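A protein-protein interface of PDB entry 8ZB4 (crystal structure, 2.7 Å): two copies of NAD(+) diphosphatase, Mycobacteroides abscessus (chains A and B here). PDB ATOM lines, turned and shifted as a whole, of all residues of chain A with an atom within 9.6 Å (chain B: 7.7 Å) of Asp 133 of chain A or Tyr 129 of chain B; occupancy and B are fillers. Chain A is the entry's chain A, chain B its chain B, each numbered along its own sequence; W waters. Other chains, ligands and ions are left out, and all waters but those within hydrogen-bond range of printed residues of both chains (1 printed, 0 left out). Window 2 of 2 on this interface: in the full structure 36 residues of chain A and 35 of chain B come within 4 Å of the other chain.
The backbone NH of Ala 127 of chain A sits close to the backbone carbonyl oxygen of Pro 131 of chain B (3.4 Å). The backbone NH (N) of Gly 128 of chain A sits at hydrogen-bond distance from the backbone carbonyl oxygen (O) of Pro 131 of chain B. The backbone NH (N) of Tyr 129 of chain A is in hydrogen-bond range of the backbone carbonyl oxygen (O) of Pro 131 of chain B (3.2 Å). The backbone carbonyl oxygen (O) of Pro 131 of chain A sits at hydrogen-bond distance from the backbone NH (N) of Gly 128 of chain B, at 3.0 Å. The backbone carbonyl oxygen of Pro 131 of chain A is in hydrogen-bond range of the backbone NH of Tyr 129 of chain B (3.2 Å). The backbone carbonyl oxygen of Asn 126 of chain A lies close to the backbone carbonyl oxygen of Pro 131 of chain B (3.4 Å). O of Asn 126 of chain B lies close to O of Pro 131 of chain A.
Printed residues of chain B within 4 Å of Asp 133 of chain A: Tyr 129 (3.0 Å). Of the printed residues of chain A, Tyr 129 of chain B touches Ser 130, Pro 131, Val 132, Asp 133 and Gly 134. Of chain A, only Pro 131 comes within 4 Å of Ala 127 of chain B. Of chain A, only Pro 131 (3.0 Å) comes within 4 Å of Gly 128 of chain B. No residue of chain A comes within 4 Å of Pro 136 of chain B. Of the printed residues of chain B, Ser 130 of chain A touches Tyr 129 (3.7 Å). Of the printed residues of chain A, Asp 133 of chain B touches Tyr 129. Of the printed residues of chain A, Gly 134 of chain B touches Tyr 129 (3.9 Å). Printed residues of chain B within 4 Å of Val 132 of chain A: Asn 126 and Tyr 129. Of the printed residues of chain B, Gly 128 of chain A touches Pro 131. Asp 125 of chain B touches none of the printed residues of chain A. The nearest residue of chain A that does not touch Tyr 129 of chain B is Tyr 129 of chain A (6.0 Å).
Ala 127 of chain A touches Pro 131 of chain B, and with the chains exchanged Pro 131 of chain A touches Ala 127 of chain B. Tyr 129 of chain A touches Ser 130 of chain B, and with the chains exchanged Ser 130 of chain A touches Tyr 129 of chain B. Tyr 129 of chain A touches Val 132 of chain B, and with the chains exchanged Val 132 of chain A touches Tyr 129 of chain B. Tyr 129 of chain A touches Gly 134 of chain B, and with the chains exchanged Gly 134 of chain A touches Tyr 129 of chain B. 15 positions are printed for both chains. Of the 18 pairs that touch across the chains among the printed residues, 18 have their exchanged pair printed and touching as well.
The backbone carbonyl oxygen of Ala 127 of chain A is in hydrogen-bond range of the side-chain hydroxyl of Thr 137 of chain A (2.8 Å). OG of Ser 130 of chain A sits at hydrogen-bond distance from N of Val 132 of chain A (2.9 Å). O of Ala 127 of chain B is in hydrogen-bond range of NE of Arg 146 of chain B (2.7 Å). N of Val 132 of chain B sits at hydrogen-bond distance from OG of Ser 130 of chain B, 2.9 Å away. N of Ser 130 of chain B lies within hydrogen-bond range of O of Ser 135 of chain B (2.9 Å). ND2 of Asn 148 of chain B sits at hydrogen-bond distance from OD2 of Asp 133 of chain B, 3.0 Å away.
Water W1 lies within hydrogen-bond range of the side-chain carboxylate of Glu 155 of chain B (3.1 Å) and the guanidinium group of Arg 158 of chain A (3.4 Å).
Hydrophobic or aromatic side chains of chain A within 4 Å of the printed part of chain B: Tyr 129 and Pro 131. Along chain B the printed residues that touch a printed residue of chain A span positions 126 to 134. Among the printed residues, no Asp or Glu carboxylate lies within 4 Å of a Lys or Arg side-chain nitrogen of the other chain.
Among the printed residues, pairs that only touch across the chains: Asn 126 of chain A with Val 132 of chain B, Tyr 129 of chain A with Ser 130 of chain B, Tyr 129 of chain A with Val 132 of chain B, Tyr 129 of chain A with Asp 133 of chain B, Tyr 129 of chain A with Gly 134 of chain B, Ser 130 of chain A with Tyr 129 of chain B, Pro 131 of chain A with Ala 127 of chain B, Val 132 of chain A with Asn 126 of chain B, Val 132 of chain A with Tyr 129 of chain B, Asp 133 of chain A with Tyr 129 of chain B and Gly 134 of chain A with Tyr 129 of chain B.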
ATOM      1  N   ASN A 126      26.606   6.321   8.138  1.00  0.00           N
ATOM      2  CA  ASN A 126      26.765   7.762   7.959  1.00  0.00           C
ATOM      3  C   ASN A 126      25.525   8.388   7.315  1.00  0.00           C
ATOM      4  O   ASN A 126      25.629   9.389   6.605  1.00  0.00           O
ATOM      5  CB  ASN A 126      27.963   8.136   7.085  1.00  0.00           C
ATOM      6  CG  ASN A 126      29.290   7.671   7.629  1.00  0.00           C
ATOM      7  OD1 ASN A 126      30.117   8.498   8.030  1.00  0.00           O
ATOM      8  ND2 ASN A 126      29.523   6.369   7.608  1.00  0.00           N
ATOM      9  N   ALA A 127      24.344   7.805   7.529  1.00  0.00           N
ATOM     10  CA  ALA A 127      23.139   8.347   6.918  1.00  0.00           C
ATOM     11  C   ALA A 127      21.926   8.114   7.817  1.00  0.00           C
ATOM     12  O   ALA A 127      20.828   7.823   7.339  1.00  0.00           O
ATOM     13  CB  ALA A 127      22.955   7.745   5.536  1.00  0.00           C
ATOM     14  N   GLY A 128      22.117   8.295   9.128  1.00  0.00           N
ATOM     15  CA  GLY A 128      21.050   8.081  10.092  1.00  0.00           C
ATOM     16  C   GLY A 128      20.186   9.332  10.261  1.00  0.00           C
ATOM     17  O   GLY A 128      19.225   9.311  11.025  1.00  0.00           O
ATOM     18  N   TYR A 129      20.543  10.409   9.540  1.00  0.00           N
ATOM     19  CA  TYR A 129      19.862  11.692   9.624  1.00  0.00           C
ATOM     20  C   TYR A 129      19.761  12.315   8.228  1.00  0.00           C
ATOM     21  O   TYR A 129      20.669  12.169   7.407  1.00  0.00           O
ATOM     22  CB  TYR A 129      20.641  12.541  10.637  1.00  0.00           C
ATOM     23  CG  TYR A 129      20.647  11.949  12.041  1.00  0.00           C
ATOM     24  CD1 TYR A 129      21.564  10.961  12.393  1.00  0.00           C
ATOM     25  CD2 TYR A 129      19.723  12.343  13.007  1.00  0.00           C
ATOM     26  CE1 TYR A 129      21.567  10.389  13.656  1.00  0.00           C
ATOM     27  CE2 TYR A 129      19.725  11.783  14.277  1.00  0.00           C
ATOM     28  CZ  TYR A 129      20.651  10.805  14.602  1.00  0.00           C
ATOM     29  OH  TYR A 129      20.677  10.244  15.843  1.00  0.00           O
ATOM     30  N   SER A 130      18.645  13.002   7.954  1.00  0.00           N
ATOM     31  CA  SER A 130      18.515  13.750   6.713  1.00  0.00           C
ATOM     32  C   SER A 130      19.484  14.930   6.712  1.00  0.00           C
ATOM     33  O   SER A 130      19.548  15.693   7.665  1.00  0.00           O
ATOM     34  CB  SER A 130      17.105  14.227   6.459  1.00  0.00           C
ATOM     35  OG  SER A 130      17.093  15.199   5.416  1.00  0.00           O
ATOM     36  N   PRO A 131      20.261  15.117   5.626  1.00  0.00           N
ATOM     37  CA  PRO A 131      21.070  16.326   5.457  1.00  0.00           C
ATOM     38  C   PRO A 131      20.239  17.552   5.103  1.00  0.00           C
ATOM     39  O   PRO A 131      20.766  18.676   5.083  1.00  0.00           O
ATOM     40  CB  PRO A 131      22.043  15.963   4.313  1.00  0.00           C
ATOM     41  CG  PRO A 131      21.364  14.854   3.563  1.00  0.00           C
ATOM     42  CD  PRO A 131      20.427  14.152   4.527  1.00  0.00           C
ATOM     43  N   VAL A 132      18.959  17.296   4.782  1.00  0.00           N
ATOM     44  CA  VAL A 132      18.053  18.329   4.318  1.00  0.00           C
ATOM     45  C   VAL A 132      17.580  19.136   5.524  1.00  0.00           C
ATOM     46  O   VAL A 132      17.857  20.329   5.596  1.00  0.00           O
ATOM     47  CB  VAL A 132      16.870  17.755   3.504  1.00  0.00           C
ATOM     48  CG1 VAL A 132      15.951  18.857   2.976  1.00  0.00           C
ATOM     49  CG2 VAL A 132      17.347  16.868   2.353  1.00  0.00           C
ATOM     50  N   ASP A 133      16.924  18.447   6.471  1.00  0.00           N
ATOM     51  CA  ASP A 133      16.261  19.063   7.614  1.00  0.00           C
ATOM     52  C   ASP A 133      16.959  18.679   8.929  1.00  0.00           C
ATOM     53  O   ASP A 133      17.152  19.537   9.786  1.00  0.00           O
ATOM     54  CB  ASP A 133      14.773  18.732   7.602  1.00  0.00           C
ATOM     55  CG  ASP A 133      14.434  17.246   7.625  1.00  0.00           C
ATOM     56  OD1 ASP A 133      15.339  16.445   7.900  1.00  0.00           O
ATOM     57  OD2 ASP A 133      13.284  16.888   7.335  1.00  0.00           O
ATOM     58  N   GLY A 134      17.315  17.394   9.101  1.00  0.00           N
ATOM     59  CA  GLY A 134      17.962  16.904  10.312  1.00  0.00           C
ATOM     60  C   GLY A 134      17.257  15.686  10.918  1.00  0.00           C
ATOM     61  O   GLY A 134      17.740  15.096  11.873  1.00  0.00           O
ATOM     62  N   SER A 135      16.099  15.299  10.390  1.00  0.00           N
ATOM     63  CA  SER A 135      15.293  14.282  11.049  1.00  0.00           C
ATOM     64  C   SER A 135      16.051  12.954  11.098  1.00  0.00           C
ATOM     65  O   SER A 135      16.842  12.669  10.212  1.00  0.00           O
ATOM     66  CB  SER A 135      13.953  14.132  10.362  1.00  0.00           C
ATOM     67  OG  SER A 135      13.346  15.404  10.172  1.00  0.00           O
ATOM     68  N   PRO A 136      15.862  12.095  12.125  1.00  0.00           N
ATOM     69  CA  PRO A 136      16.262  10.685  12.023  1.00  0.00           C
ATOM     70  C   PRO A 136      15.758  10.066  10.723  1.00  0.00           C
ATOM     71  O   PRO A 136      14.770  10.557  10.197  1.00  0.00           O
ATOM     72  CB  PRO A 136      15.644   9.996  13.269  1.00  0.00           C
ATOM     73  CG  PRO A 136      14.957  11.105  14.065  1.00  0.00           C
ATOM     74  CD  PRO A 136      15.362  12.451  13.462  1.00  0.00           C
ATOM     75  N   THR A 137      16.420   8.991  10.248  1.00  0.00           N
ATOM     76  CA  THR A 137      16.021   8.246   9.057  1.00  0.00           C
ATOM     77  C   THR A 137      15.940   6.768   9.420  1.00  0.00           C
ATOM     78  O   THR A 137      16.538   6.361  10.401  1.00  0.00           O
ATOM     79  CB  THR A 137      17.015   8.460   7.913  1.00  0.00           C
ATOM     80  OG1 THR A 137      18.215   7.777   8.265  1.00  0.00           O
ATOM     81  CG2 THR A 137      17.349   9.922   7.649  1.00  0.00           C
ATOM     82  N   VAL A 147      14.352   6.072   4.877  1.00  0.00           N
ATOM     83  CA  VAL A 147      13.226   6.993   4.840  1.00  0.00           C
ATOM     84  C   VAL A 147      13.323   7.977   6.001  1.00  0.00           C
ATOM     85  O   VAL A 147      13.579   7.577   7.131  1.00  0.00           O
ATOM     86  CB  VAL A 147      11.895   6.224   4.906  1.00  0.00           C
ATOM     87  CG1 VAL A 147      10.707   7.160   5.078  1.00  0.00           C
ATOM     88  CG2 VAL A 147      11.698   5.331   3.689  1.00  0.00           C
ATOM     89  N   ASN A 148      13.078   9.257   5.699  1.00  0.00           N
ATOM     90  CA  ASN A 148      12.977  10.318   6.690  1.00  0.00           C
ATOM     91  C   ASN A 148      11.736  10.081   7.566  1.00  0.00           C
ATOM     92  O   ASN A 148      10.703   9.610   7.085  1.00  0.00           O
ATOM     93  CB  ASN A 148      12.996  11.672   5.973  1.00  0.00           C
ATOM     94  CG  ASN A 148      12.808  12.841   6.904  1.00  0.00           C
ATOM     95  OD1 ASN A 148      12.024  12.739   7.853  1.00  0.00           O
ATOM     96  ND2 ASN A 148      13.523  13.936   6.670  1.00  0.00           N
ATOM     97  N   SER A 149      11.848  10.420   8.862  1.00  0.00           N
ATOM     98  CA  SER A 149      10.827  10.117   9.862  1.00  0.00           C
ATOM     99  C   SER A 149       9.683  11.131   9.809  1.00  0.00           C
ATOM    100  O   SER A 149       8.511  10.758   9.819  1.00  0.00           O
ATOM    101  CB  SER A 149      11.423  10.065  11.251  1.00  0.00           C
ATOM    102  OG  SER A 149      12.027   8.806  11.501  1.00  0.00           O
ATOM    103  N   ALA A 150      10.051  12.417   9.784  1.00  0.00           N
ATOM    104  CA  ALA A 150       9.121  13.520   9.619  1.00  0.00           C
ATOM    105  C   ALA A 150       8.398  13.462   8.264  1.00  0.00           C
ATOM    106  O   ALA A 150       7.181  13.280   8.235  1.00  0.00           O
ATOM    107  CB  ALA A 150       9.879  14.825   9.809  1.00  0.00           C
ATOM    108  N   THR A 151       9.152  13.589   7.152  1.00  0.00           N
ATOM    109  CA  THR A 151       8.602  13.944   5.846  1.00  0.00           C
ATOM    110  C   THR A 151       8.350  12.729   4.946  1.00  0.00           C
ATOM    111  O   THR A 151       7.647  12.860   3.950  1.00  0.00           O
ATOM    112  CB  THR A 151       9.524  14.929   5.123  1.00  0.00           C
ATOM    113  OG1 THR A 151      10.616  14.167   4.617  1.00  0.00           O
ATOM    114  CG2 THR A 151      10.014  16.069   6.000  1.00  0.00           C
ATOM    115  N   GLY A 152       8.959  11.569   5.219  1.00  0.00           N
ATOM    116  CA  GLY A 152       8.762  10.401   4.364  1.00  0.00           C
ATOM    117  C   GLY A 152       9.670  10.389   3.129  1.00  0.00           C
ATOM    118  O   GLY A 152       9.608   9.455   2.325  1.00  0.00           O
ATOM    119  N   GLN A 153      10.533  11.408   2.985  1.00  0.00           N
ATOM    120  CA  GLN A 153      11.450  11.487   1.856  1.00  0.00           C
ATOM    121  C   GLN A 153      12.529  10.397   1.927  1.00  0.00           C
ATOM    122  O   GLN A 153      13.113  10.147   2.979  1.00  0.00           O
ATOM    123  CB  GLN A 153      12.108  12.868   1.805  1.00  0.00           C
ATOM    124  CG  GLN A 153      13.381  12.918   0.964  1.00  0.00           C
ATOM    125  CD  GLN A 153      13.738  14.294   0.436  1.00  0.00           C
ATOM    126  OE1 GLN A 153      13.708  14.529  -0.777  1.00  0.00           O
ATOM    127  NE2 GLN A 153      14.089  15.220   1.319  1.00  0.00           N
ATOM    128  N   GLU A 155      16.237   8.819   1.195  1.00  0.00           N
ATOM    129  CA  GLU A 155      17.649   9.089   0.960  1.00  0.00           C
ATOM    130  C   GLU A 155      18.306   7.822   0.413  1.00  0.00           C
ATOM    131  O   GLU A 155      17.868   6.713   0.738  1.00  0.00           O
ATOM    132  CB  GLU A 155      18.301   9.586   2.251  1.00  0.00           C
ATOM    133  CG  GLU A 155      17.796  10.963   2.672  1.00  0.00           C
ATOM    134  CD  GLU A 155      18.487  12.127   1.994  1.00  0.00           C
ATOM    135  OE1 GLU A 155      17.898  13.216   2.037  1.00  0.00           O
ATOM    136  OE2 GLU A 155      19.611  11.986   1.464  1.00  0.00           O
ATOM    137  N   ARG A 158      25.417   6.873  -1.399  1.00  0.00           N
ATOM    138  CA  ARG A 158      26.266   7.867  -2.038  1.00  0.00           C
ATOM    139  C   ARG A 158      27.574   7.240  -2.535  1.00  0.00           C
ATOM    140  O   ARG A 158      28.375   6.778  -1.736  1.00  0.00           O
ATOM    141  CB  ARG A 158      26.551   8.984  -1.028  1.00  0.00           C
ATOM    142  CG  ARG A 158      27.661   9.931  -1.466  1.00  0.00           C
ATOM    143  CD  ARG A 158      27.746  11.196  -0.605  1.00  0.00           C
ATOM    144  NE  ARG A 158      28.778  12.121  -1.094  1.00  0.00           N
ATOM    145  CZ  ARG A 158      28.902  13.384  -0.718  1.00  0.00           C
ATOM    146  NH1 ARG A 158      28.106  13.881   0.208  1.00  0.00           N
ATOM    147  NH2 ARG A 158      29.813  14.159  -1.278  1.00  0.00           N
ATOM    148  N   HIS B 124      24.091  23.138  -1.155  1.00  0.00           N
ATOM    149  CA  HIS B 124      23.956  23.843   0.112  1.00  0.00           C
ATOM    150  C   HIS B 124      22.522  23.748   0.624  1.00  0.00           C
ATOM    151  O   HIS B 124      22.302  23.391   1.779  1.00  0.00           O
ATOM    152  CB  HIS B 124      24.394  25.303  -0.004  1.00  0.00           C
ATOM    153  CG  HIS B 124      25.873  25.482  -0.030  1.00  0.00           C
ATOM    154  ND1 HIS B 124      26.729  25.163   1.002  1.00  0.00           N
ATOM    155  CD2 HIS B 124      26.635  25.952  -1.024  1.00  0.00           C
ATOM    156  CE1 HIS B 124      27.969  25.453   0.629  1.00  0.00           C
ATOM    157  NE2 HIS B 124      27.928  25.947  -0.592  1.00  0.00           N
ATOM    158  N   ASP B 125      21.544  24.006  -0.250  1.00  0.00           N
ATOM    159  CA  ASP B 125      20.156  23.981   0.172  1.00  0.00           C
ATOM    160  C   ASP B 125      19.768  22.606   0.713  1.00  0.00           C
ATOM    161  O   ASP B 125      18.790  22.516   1.443  1.00  0.00           O
ATOM    162  CB  ASP B 125      19.215  24.430  -0.933  1.00  0.00           C
ATOM    163  CG  ASP B 125      19.338  25.880  -1.376  1.00  0.00           C
ATOM    164  OD1 ASP B 125      20.105  26.652  -0.754  1.00  0.00           O
ATOM    165  OD2 ASP B 125      18.675  26.214  -2.360  1.00  0.00           O
ATOM    166  N   ASN B 126      20.509  21.536   0.378  1.00  0.00           N
ATOM    167  CA  ASN B 126      20.140  20.206   0.849  1.00  0.00           C
ATOM    168  C   ASN B 126      21.205  19.594   1.756  1.00  0.00           C
ATOM    169  O   ASN B 126      21.161  18.390   1.981  1.00  0.00           O
ATOM    170  CB  ASN B 126      19.855  19.225  -0.290  1.00  0.00           C
ATOM    171  CG  ASN B 126      18.688  19.639  -1.158  1.00  0.00           C
ATOM    172  OD1 ASN B 126      17.623  19.012  -1.129  1.00  0.00           O
ATOM    173  ND2 ASN B 126      18.868  20.686  -1.947  1.00  0.00           N
ATOM    174  N   ALA B 127      22.090  20.410   2.339  1.00  0.00           N
ATOM    175  CA  ALA B 127      23.185  19.883   3.138  1.00  0.00           C
ATOM    176  C   ALA B 127      23.434  20.751   4.375  1.00  0.00           C
ATOM    177  O   ALA B 127      24.575  21.002   4.757  1.00  0.00           O
ATOM    178  CB  ALA B 127      24.417  19.774   2.261  1.00  0.00           C
ATOM    179  N   GLY B 128      22.348  21.167   5.029  1.00  0.00           N
ATOM    180  CA  GLY B 128      22.444  22.036   6.191  1.00  0.00           C
ATOM    181  C   GLY B 128      22.631  21.240   7.479  1.00  0.00           C
ATOM    182  O   GLY B 128      22.728  21.831   8.545  1.00  0.00           O
ATOM    183  N   TYR B 129      22.674  19.908   7.364  1.00  0.00           N
ATOM    184  CA  TYR B 129      22.788  19.018   8.507  1.00  0.00           C
ATOM    185  C   TYR B 129      23.701  17.843   8.152  1.00  0.00           C
ATOM    186  O   TYR B 129      23.702  17.366   7.016  1.00  0.00           O
ATOM    187  CB  TYR B 129      21.381  18.582   8.938  1.00  0.00           C
ATOM    188  CG  TYR B 129      20.488  19.749   9.333  1.00  0.00           C
ATOM    189  CD1 TYR B 129      19.835  20.511   8.369  1.00  0.00           C
ATOM    190  CD2 TYR B 129      20.310  20.102  10.667  1.00  0.00           C
ATOM    191  CE1 TYR B 129      19.043  21.593   8.718  1.00  0.00           C
ATOM    192  CE2 TYR B 129      19.511  21.178  11.030  1.00  0.00           C
ATOM    193  CZ  TYR B 129      18.877  21.926  10.051  1.00  0.00           C
ATOM    194  OH  TYR B 129      18.078  22.984  10.377  1.00  0.00           O
ATOM    195  N   SER B 130      24.502  17.393   9.131  1.00  0.00           N
ATOM    196  CA  SER B 130      25.270  16.173   8.958  1.00  0.00           C
ATOM    197  C   SER B 130      24.322  14.980   8.880  1.00  0.00           C
ATOM    198  O   SER B 130      23.435  14.821   9.718  1.00  0.00           O
ATOM    199  CB  SER B 130      26.285  15.959  10.041  1.00  0.00           C
ATOM    200  OG  SER B 130      26.768  14.618  10.010  1.00  0.00           O
ATOM    201  N   PRO B 131      24.489  14.105   7.864  1.00  0.00           N
ATOM    202  CA  PRO B 131      23.759  12.841   7.815  1.00  0.00           C
ATOM    203  C   PRO B 131      24.278  11.816   8.819  1.00  0.00           C
ATOM    204  O   PRO B 131      23.659  10.762   9.005  1.00  0.00           O
ATOM    205  CB  PRO B 131      23.958  12.375   6.356  1.00  0.00           C
ATOM    206  CG  PRO B 131      25.242  13.033   5.906  1.00  0.00           C
ATOM    207  CD  PRO B 131      25.358  14.317   6.696  1.00  0.00           C
ATOM    208  N   VAL B 132      25.431  12.142   9.424  1.00  0.00           N
ATOM    209  CA  VAL B 132      26.130  11.237  10.321  1.00  0.00           C
ATOM    210  C   VAL B 132      25.430  11.269  11.674  1.00  0.00           C
ATOM    211  O   VAL B 132      24.912  10.244  12.116  1.00  0.00           O
ATOM    212  CB  VAL B 132      27.630  11.583  10.443  1.00  0.00           C
ATOM    213  CG1 VAL B 132      28.371  10.599  11.345  1.00  0.00           C
ATOM    214  CG2 VAL B 132      28.309  11.670   9.075  1.00  0.00           C
ATOM    215  N   ASP B 133      25.371  12.466  12.278  1.00  0.00           N
ATOM    216  CA  ASP B 133      24.866  12.659  13.633  1.00  0.00           C
ATOM    217  C   ASP B 133      23.543  13.440  13.639  1.00  0.00           C
ATOM    218  O   ASP B 133      22.633  13.087  14.389  1.00  0.00           O
ATOM    219  CB  ASP B 133      25.938  13.291  14.514  1.00  0.00           C
ATOM    220  CG  ASP B 133      26.489  14.618  14.016  1.00  0.00           C
ATOM    221  OD1 ASP B 133      25.855  15.209  13.124  1.00  0.00           O
ATOM    222  OD2 ASP B 133      27.555  15.041  14.498  1.00  0.00           O
ATOM    223  N   GLY B 134      23.454  14.514  12.835  1.00  0.00           N
ATOM    224  CA  GLY B 134      22.273  15.364  12.777  1.00  0.00           C
ATOM    225  C   GLY B 134      22.579  16.839  13.054  1.00  0.00           C
ATOM    226  O   GLY B 134      21.691  17.688  12.964  1.00  0.00           O
ATOM    227  N   SER B 135      23.830  17.168  13.390  1.00  0.00           N
ATOM    228  CA  SER B 135      24.150  18.532  13.780  1.00  0.00           C
ATOM    229  C   SER B 135      23.894  19.473  12.605  1.00  0.00           C
ATOM    230  O   SER B 135      23.819  19.031  11.476  1.00  0.00           O
ATOM    231  CB  SER B 135      25.571  18.642  14.292  1.00  0.00           C
ATOM    232  OG  SER B 135      25.840  17.624  15.248  1.00  0.00           O
ATOM    233  N   PRO B 136      23.559  20.758  12.836  1.00  0.00           N
ATOM    234  CA  PRO B 136      23.716  21.793  11.809  1.00  0.00           C
ATOM    235  C   PRO B 136      25.099  21.770  11.181  1.00  0.00           C
ATOM    236  O   PRO B 136      26.012  21.274  11.815  1.00  0.00           O
ATOM    237  CB  PRO B 136      23.482  23.080  12.619  1.00  0.00           C
ATOM    238  CG  PRO B 136      22.445  22.655  13.628  1.00  0.00           C
ATOM    239  CD  PRO B 136      22.842  21.241  14.026  1.00  0.00           C
ATOM    240  N   THR B 137      25.239  22.351   9.975  1.00  0.00           N
ATOM    241  CA  THR B 137      26.517  22.503   9.278  1.00  0.00           C
ATOM    242  C   THR B 137      26.656  23.958   8.838  1.00  0.00           C
ATOM    243  O   THR B 137      25.653  24.639   8.734  1.00  0.00           O
ATOM    244  CB  THR B 137      26.608  21.571   8.061  1.00  0.00           C
ATOM    245  OG1 THR B 137      25.705  22.059   7.074  1.00  0.00           O
ATOM    246  CG2 THR B 137      26.269  20.121   8.364  1.00  0.00           C
ATOM    247  N   ILE B 138      27.869  24.402   8.483  1.00  0.00           N
ATOM    248  CA  ILE B 138      28.124  25.816   8.224  1.00  0.00           C
ATOM    249  C   ILE B 138      28.967  25.956   6.963  1.00  0.00           C
ATOM    250  O   ILE B 138      30.029  25.357   6.888  1.00  0.00           O
ATOM    251  CB  ILE B 138      28.896  26.491   9.384  1.00  0.00           C
ATOM    252  CG1 ILE B 138      28.524  25.998  10.805  1.00  0.00           C
ATOM    253  CG2 ILE B 138      28.829  28.011   9.261  1.00  0.00           C
ATOM    254  CD1 ILE B 138      27.166  26.442  11.300  1.00  0.00           C
ATOM    255  N   ARG B 146      30.899  22.377   3.806  1.00  0.00           N
ATOM    256  CA  ARG B 146      30.145  22.748   4.987  1.00  0.00           C
ATOM    257  C   ARG B 146      30.696  21.980   6.188  1.00  0.00           C
ATOM    258  O   ARG B 146      30.737  20.751   6.174  1.00  0.00           O
ATOM    259  CB  ARG B 146      28.651  22.452   4.837  1.00  0.00           C
ATOM    260  CG  ARG B 146      27.954  23.266   3.759  1.00  0.00           C
ATOM    261  CD  ARG B 146      26.476  22.894   3.722  1.00  0.00           C
ATOM    262  NE  ARG B 146      25.672  23.491   4.797  1.00  0.00           N
ATOM    263  CZ  ARG B 146      25.186  24.733   4.801  1.00  0.00           C
ATOM    264  NH1 ARG B 146      25.439  25.566   3.801  1.00  0.00           N
ATOM    265  NH2 ARG B 146      24.442  25.136   5.814  1.00  0.00           N
ATOM    266  N   ASN B 148      30.680  20.700  10.109  1.00  0.00           N
ATOM    267  CA  ASN B 148      29.773  20.314  11.180  1.00  0.00           C
ATOM    268  C   ASN B 148      30.011  21.225  12.392  1.00  0.00           C
ATOM    269  O   ASN B 148      31.141  21.624  12.662  1.00  0.00           O
ATOM    270  CB  ASN B 148      29.909  18.822  11.459  1.00  0.00           C
ATOM    271  CG  ASN B 148      29.063  18.357  12.620  1.00  0.00           C
ATOM    272  OD1 ASN B 148      28.933  19.086  13.608  1.00  0.00           O
ATOM    273  ND2 ASN B 148      28.483  17.165  12.543  1.00  0.00           N
ATOM    274  N   SER B 149      28.929  21.552  13.116  1.00  0.00           N
ATOM    275  CA  SER B 149      28.943  22.532  14.199  1.00  0.00           C
ATOM    276  C   SER B 149      29.490  21.919  15.489  1.00  0.00           C
ATOM    277  O   SER B 149      30.329  22.518  16.154  1.00  0.00           O
ATOM    278  CB  SER B 149      27.555  23.128  14.410  1.00  0.00           C
ATOM    279  OG  SER B 149      26.531  22.139  14.463  1.00  0.00           O
ATOM    280  N   GLU B 155      31.775  18.225   5.259  1.00  0.00           N
ATOM    281  CA  GLU B 155      30.922  17.609   4.250  1.00  0.00           C
ATOM    282  C   GLU B 155      31.228  18.295   2.920  1.00  0.00           C
ATOM    283  O   GLU B 155      31.541  19.481   2.890  1.00  0.00           O
ATOM    284  CB  GLU B 155      29.445  17.707   4.638  1.00  0.00           C
ATOM    285  CG  GLU B 155      29.105  16.949   5.918  1.00  0.00           C
ATOM    286  CD  GLU B 155      28.846  15.470   5.719  1.00  0.00           C
ATOM    287  OE1 GLU B 155      29.021  14.720   6.702  1.00  0.00           O
ATOM    288  OE2 GLU B 155      28.462  15.059   4.597  1.00  0.00           O
HETATM  289  O   HOH W   1      30.484  15.202   2.217  1.00  0.00           O
